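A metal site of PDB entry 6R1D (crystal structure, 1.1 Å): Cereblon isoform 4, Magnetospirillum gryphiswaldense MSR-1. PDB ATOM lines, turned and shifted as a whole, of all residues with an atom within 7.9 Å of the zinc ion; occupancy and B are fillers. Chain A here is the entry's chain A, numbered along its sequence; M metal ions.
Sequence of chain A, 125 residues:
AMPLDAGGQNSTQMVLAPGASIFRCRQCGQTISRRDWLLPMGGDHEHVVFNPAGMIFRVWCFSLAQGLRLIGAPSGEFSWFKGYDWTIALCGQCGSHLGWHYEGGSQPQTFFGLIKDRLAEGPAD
The zinc ion is bound by SG of Cys 94 (2.3 Å), SG of Cys 28 (2.3 Å), SG of Cys 91 (2.3 Å) and SG of Cys 25 (2.4 Å).
The backbone NH of Gln 27 sits close to the side-chain sulfur of Cys 25 (3.5 Å). The side-chain sulfur (SG) of Cys 91 sits close to the backbone NH (N) of Gln 93. O of Gln 30 sits at hydrogen-bond distance from N of Cys 25, at 2.8 Å. The side-chain sulfur (SG) of Cys 94 lies close to the side-chain hydroxyl (OG) of Ser 96. O of Ser 96 sits at hydrogen-bond distance from N of Cys 91 (2.8 Å). SG of Cys 28 lies close to N of Gln 30.
Within 4 Å of the zinc ion: Cys 25, Cys 28, Cys 91 and Cys 94.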
ATOM      1  N   ARG A  24     -28.713 -25.749  12.368  1.00  0.00           N
ATOM      2  CA  ARG A  24     -29.567 -26.441  13.333  1.00  0.00           C
ATOM      3  C   ARG A  24     -28.787 -27.654  13.899  1.00  0.00           C
ATOM      4  O   ARG A  24     -27.910 -28.176  13.262  1.00  0.00           O
ATOM      5  CB  ARG A  24     -30.846 -26.918  12.606  1.00  0.00           C
ATOM      6  CG  ARG A  24     -31.715 -25.808  12.138  1.00  0.00           C
ATOM      7  CD  ARG A  24     -32.917 -26.299  11.374  1.00  0.00           C
ATOM      8  NE  ARG A  24     -33.819 -25.250  11.018  1.00  0.00           N
ATOM      9  CZ  ARG A  24     -33.797 -24.505   9.887  1.00  0.00           C
ATOM     10  NH1 ARG A  24     -32.824 -24.712   8.986  1.00  0.00           N
ATOM     11  NH2 ARG A  24     -34.696 -23.585   9.655  1.00  0.00           N
ATOM     12  N   CYS A  25     -29.226 -28.105  15.055  1.00  0.00           N
ATOM     13  CA  CYS A  25     -28.752 -29.326  15.605  1.00  0.00           C
ATOM     14  C   CYS A  25     -29.085 -30.431  14.670  1.00  0.00           C
ATOM     15  O   CYS A  25     -30.258 -30.616  14.281  1.00  0.00           O
ATOM     16  CB  CYS A  25     -29.372 -29.609  16.971  1.00  0.00           C
ATOM     17  SG  CYS A  25     -28.959 -31.200  17.656  1.00  0.00           S
ATOM     18  N   ARG A  26     -28.104 -31.239  14.270  1.00  0.00           N
ATOM     19  CA  ARG A  26     -28.332 -32.323  13.378  1.00  0.00           C
ATOM     20  C   ARG A  26     -29.191 -33.441  13.905  1.00  0.00           C
ATOM     21  O   ARG A  26     -29.927 -34.102  13.221  1.00  0.00           O
ATOM     22  CB  ARG A  26     -27.021 -32.971  12.917  1.00  0.00           C
ATOM     23  CG  ARG A  26     -27.206 -33.707  11.677  1.00  0.00           C
ATOM     24  CD  ARG A  26     -25.868 -34.091  11.024  1.00  0.00           C
ATOM     25  NE  ARG A  26     -25.021 -33.255  10.163  1.00  0.00           N
ATOM     26  CZ  ARG A  26     -25.306 -32.749   8.894  1.00  0.00           C
ATOM     27  NH1 ARG A  26     -24.271 -32.240   8.222  1.00  0.00           N
ATOM     28  NH2 ARG A  26     -26.497 -32.586   8.356  1.00  0.00           N
ATOM     29  N   GLN A  27     -29.162 -33.620  15.197  1.00  0.00           N
ATOM     30  CA  GLN A  27     -29.957 -34.668  15.867  1.00  0.00           C
ATOM     31  C   GLN A  27     -31.432 -34.309  16.036  1.00  0.00           C
ATOM     32  O   GLN A  27     -32.280 -35.159  15.794  1.00  0.00           O
ATOM     33  CB  GLN A  27     -29.418 -34.959  17.284  1.00  0.00           C
ATOM     34  CG  GLN A  27     -29.998 -36.192  17.875  1.00  0.00           C
ATOM     35  CD  GLN A  27     -29.567 -36.509  19.329  1.00  0.00           C
ATOM     36  OE1 GLN A  27     -30.454 -36.929  20.121  1.00  0.00           O
ATOM     37  NE2 GLN A  27     -28.303 -36.463  19.625  1.00  0.00           N
ATOM     38  N   CYS A  28     -31.746 -33.076  16.399  1.00  0.00           N
ATOM     39  CA  CYS A  28     -33.122 -32.754  16.758  1.00  0.00           C
ATOM     40  C   CYS A  28     -33.703 -31.598  15.982  1.00  0.00           C
ATOM     41  O   CYS A  28     -34.937 -31.366  16.076  1.00  0.00           O
ATOM     42  CB  CYS A  28     -33.288 -32.499  18.246  1.00  0.00           C
ATOM     43  SG  CYS A  28     -32.686 -30.900  18.788  1.00  0.00           S
ATOM     44  N   GLY A  29     -32.892 -30.833  15.252  1.00  0.00           N
ATOM     45  CA  GLY A  29     -33.360 -29.707  14.507  1.00  0.00           C
ATOM     46  C   GLY A  29     -33.488 -28.378  15.230  1.00  0.00           C
ATOM     47  O   GLY A  29     -33.846 -27.373  14.636  1.00  0.00           O
ATOM     48  N   GLN A  30     -33.091 -28.347  16.491  1.00  0.00           N
ATOM     49  CA  GLN A  30     -33.036 -27.158  17.233  1.00  0.00           C
ATOM     50  C   GLN A  30     -32.225 -26.068  16.471  1.00  0.00           C
ATOM     51  O   GLN A  30     -31.124 -26.321  15.988  1.00  0.00           O
ATOM     52  CB  GLN A  30     -32.266 -27.401  18.563  1.00  0.00           C
ATOM     53  CG  GLN A  30     -31.966 -26.294  19.573  1.00  0.00           C
ATOM     54  CD  GLN A  30     -33.016 -26.067  20.569  1.00  0.00           C
ATOM     55  OE1 GLN A  30     -34.200 -26.301  20.337  1.00  0.00           O
ATOM     56  NE2 GLN A  30     -32.573 -25.797  21.842  1.00  0.00           N
ATOM     57  N   THR A  31     -32.735 -24.854  16.384  1.00  0.00           N
ATOM     58  CA  THR A  31     -32.011 -23.776  15.739  1.00  0.00           C
ATOM     59  C   THR A  31     -30.867 -23.301  16.610  1.00  0.00           C
ATOM     60  O   THR A  31     -31.073 -23.054  17.772  1.00  0.00           O
ATOM     61  CB  THR A  31     -32.925 -22.615  15.407  1.00  0.00           C
ATOM     62  OG1 THR A  31     -33.956 -23.136  14.615  1.00  0.00           O
ATOM     63  CG2 THR A  31     -32.204 -21.549  14.708  1.00  0.00           C
ATOM     64  N   ILE A  32     -29.678 -23.143  16.044  1.00  0.00           N
ATOM     65  CA  ILE A  32     -28.473 -22.812  16.802  1.00  0.00           C
ATOM     66  C   ILE A  32     -27.805 -21.526  16.341  1.00  0.00           C
ATOM     67  O   ILE A  32     -27.535 -20.662  17.148  1.00  0.00           O
ATOM     68  CB  ILE A  32     -27.456 -23.967  16.753  1.00  0.00           C
ATOM     69  CG1 ILE A  32     -28.055 -25.294  17.210  1.00  0.00           C
ATOM     70  CG2 ILE A  32     -26.233 -23.594  17.577  1.00  0.00           C
ATOM     71  CD1 ILE A  32     -28.524 -25.370  18.649  1.00  0.00           C
ATOM     72  N   GLY A  67     -29.969 -21.706  21.638  1.00  0.00           N
ATOM     73  CA  GLY A  67     -30.381 -23.056  21.697  1.00  0.00           C
ATOM     74  C   GLY A  67     -29.453 -23.996  22.423  1.00  0.00           C
ATOM     75  O   GLY A  67     -29.678 -25.191  22.360  1.00  0.00           O
ATOM     76  N   LEU A  90     -23.940 -28.035  24.998  1.00  0.00           N
ATOM     77  CA  LEU A  90     -24.872 -29.054  24.559  1.00  0.00           C
ATOM     78  C   LEU A  90     -26.054 -28.434  23.857  1.00  0.00           C
ATOM     79  O   LEU A  90     -26.402 -27.295  24.130  1.00  0.00           O
ATOM     80  CB  LEU A  90     -25.444 -29.804  25.737  1.00  0.00           C
ATOM     81  CG  LEU A  90     -24.453 -30.526  26.665  1.00  0.00           C
ATOM     82  CD1 LEU A  90     -25.225 -31.208  27.787  1.00  0.00           C
ATOM     83  CD2 LEU A  90     -23.535 -31.475  25.905  1.00  0.00           C
ATOM     84  N   CYS A  91     -26.669 -29.164  22.928  1.00  0.00           N
ATOM     85  CA  CYS A  91     -27.994 -28.780  22.451  1.00  0.00           C
ATOM     86  C   CYS A  91     -28.917 -28.692  23.686  1.00  0.00           C
ATOM     87  O   CYS A  91     -29.054 -29.702  24.405  1.00  0.00           O
ATOM     88  CB  CYS A  91     -28.454 -29.801  21.446  1.00  0.00           C
ATOM     89  SG  CYS A  91     -30.143 -29.355  20.861  1.00  0.00           S
ATOM     90  N   GLY A  92     -29.636 -27.595  23.831  1.00  0.00           N
ATOM     91  CA  GLY A  92     -30.529 -27.448  24.932  1.00  0.00           C
ATOM     92  C   GLY A  92     -31.770 -28.291  24.863  1.00  0.00           C
ATOM     93  O   GLY A  92     -32.434 -28.462  25.872  1.00  0.00           O
ATOM     94  N   GLN A  93     -32.046 -28.859  23.685  1.00  0.00           N
ATOM     95  CA  GLN A  93     -33.219 -29.747  23.466  1.00  0.00           C
ATOM     96  C   GLN A  93     -32.860 -31.178  23.658  1.00  0.00           C
ATOM     97  O   GLN A  93     -33.589 -31.847  24.347  1.00  0.00           O
ATOM     98  CB  GLN A  93     -33.877 -29.434  22.073  1.00  0.00           C
ATOM     99  CG  GLN A  93     -35.022 -30.361  21.779  1.00  0.00           C
ATOM    100  CD  GLN A  93     -36.181 -30.084  22.704  1.00  0.00           C
ATOM    101  OE1 GLN A  93     -36.381 -28.927  23.176  1.00  0.00           O
ATOM    102  NE2 GLN A  93     -37.029 -31.138  22.955  1.00  0.00           N
ATOM    103  N   CYS A  94     -31.839 -31.669  22.991  1.00  0.00           N
ATOM    104  CA  CYS A  94     -31.570 -33.105  22.891  1.00  0.00           C
ATOM    105  C   CYS A  94     -30.322 -33.557  23.589  1.00  0.00           C
ATOM    106  O   CYS A  94     -30.081 -34.774  23.666  1.00  0.00           O
ATOM    107  CB  CYS A  94     -31.548 -33.618  21.456  1.00  0.00           C
ATOM    108  SG  CYS A  94     -30.050 -33.162  20.548  1.00  0.00           S
ATOM    109  N   GLY A  95     -29.506 -32.634  24.071  1.00  0.00           N
ATOM    110  CA  GLY A  95     -28.295 -33.015  24.743  1.00  0.00           C
ATOM    111  C   GLY A  95     -27.137 -33.423  23.920  1.00  0.00           C
ATOM    112  O   GLY A  95     -26.100 -33.797  24.450  1.00  0.00           O
ATOM    113  N   SER A  96     -27.215 -33.317  22.593  1.00  0.00           N
ATOM    114  CA  SER A  96     -26.056 -33.547  21.751  1.00  0.00           C
ATOM    115  C   SER A  96     -24.925 -32.586  22.067  1.00  0.00           C
ATOM    116  O   SER A  96     -25.166 -31.435  22.424  1.00  0.00           O
ATOM    117  CB  SER A  96     -26.446 -33.420  20.270  1.00  0.00           C
ATOM    118  OG  SER A  96     -27.214 -34.558  19.956  1.00  0.00           O
ATOM    119  N   HIS A  97     -23.715 -33.082  21.955  1.00  0.00           N
ATOM    120  CA  HIS A  97     -22.566 -32.225  22.190  1.00  0.00           C
ATOM    121  C   HIS A  97     -22.296 -31.435  20.941  1.00  0.00           C
ATOM    122  O   HIS A  97     -21.824 -31.978  19.942  1.00  0.00           O
ATOM    123  CB  HIS A  97     -21.369 -33.062  22.606  1.00  0.00           C
ATOM    124  CG  HIS A  97     -20.107 -32.239  22.728  1.00  0.00           C
ATOM    125  ND1 HIS A  97     -18.889 -32.729  22.348  1.00  0.00           N
ATOM    126  CD2 HIS A  97     -19.946 -30.948  23.117  1.00  0.00           C
ATOM    127  CE1 HIS A  97     -18.018 -31.711  22.530  1.00  0.00           C
ATOM    128  NE2 HIS A  97     -18.628 -30.649  22.995  1.00  0.00           N
ATOM    129  N   LEU A  98     -22.619 -30.141  20.964  1.00  0.00           N
ATOM    130  CA  LEU A  98     -22.483 -29.315  19.750  1.00  0.00           C
ATOM    131  C   LEU A  98     -21.206 -28.523  19.698  1.00  0.00           C
ATOM    132  O   LEU A  98     -20.870 -27.997  18.665  1.00  0.00           O
ATOM    133  CB  LEU A  98     -23.691 -28.380  19.638  1.00  0.00           C
ATOM    134  CG  LEU A  98     -25.016 -29.129  19.376  1.00  0.00           C
ATOM    135  CD1 LEU A  98     -26.112 -28.101  19.125  1.00  0.00           C
ATOM    136  CD2 LEU A  98     -24.960 -30.184  18.360  1.00  0.00           C
ATOM    137  N   ARG A 118     -21.967 -31.852  13.527  1.00  0.00           N
ATOM    138  CA  ARG A 118     -23.102 -32.019  14.422  1.00  0.00           C
ATOM    139  C   ARG A 118     -24.225 -30.984  14.117  1.00  0.00           C
ATOM    140  O   ARG A 118     -25.211 -30.993  14.842  1.00  0.00           O
ATOM    141  CB  ARG A 118     -22.684 -31.880  15.857  1.00  0.00           C
ATOM    142  CG  ARG A 118     -21.669 -32.953  16.304  1.00  0.00           C
ATOM    143  CD  ARG A 118     -22.060 -33.854  17.224  1.00  0.00           C
ATOM    144  NE  ARG A 118     -21.007 -34.879  17.318  1.00  0.00           N
ATOM    145  CZ  ARG A 118     -20.155 -35.048  18.298  1.00  0.00           C
ATOM    146  NH1 ARG A 118     -20.157 -34.294  19.334  1.00  0.00           N
ATOM    147  NH2 ARG A 118     -19.299 -36.091  18.238  1.00  0.00           N
HETATM  148 ZN    ZN M   1     -30.486 -31.180  19.455  1.00  0.00          ZN
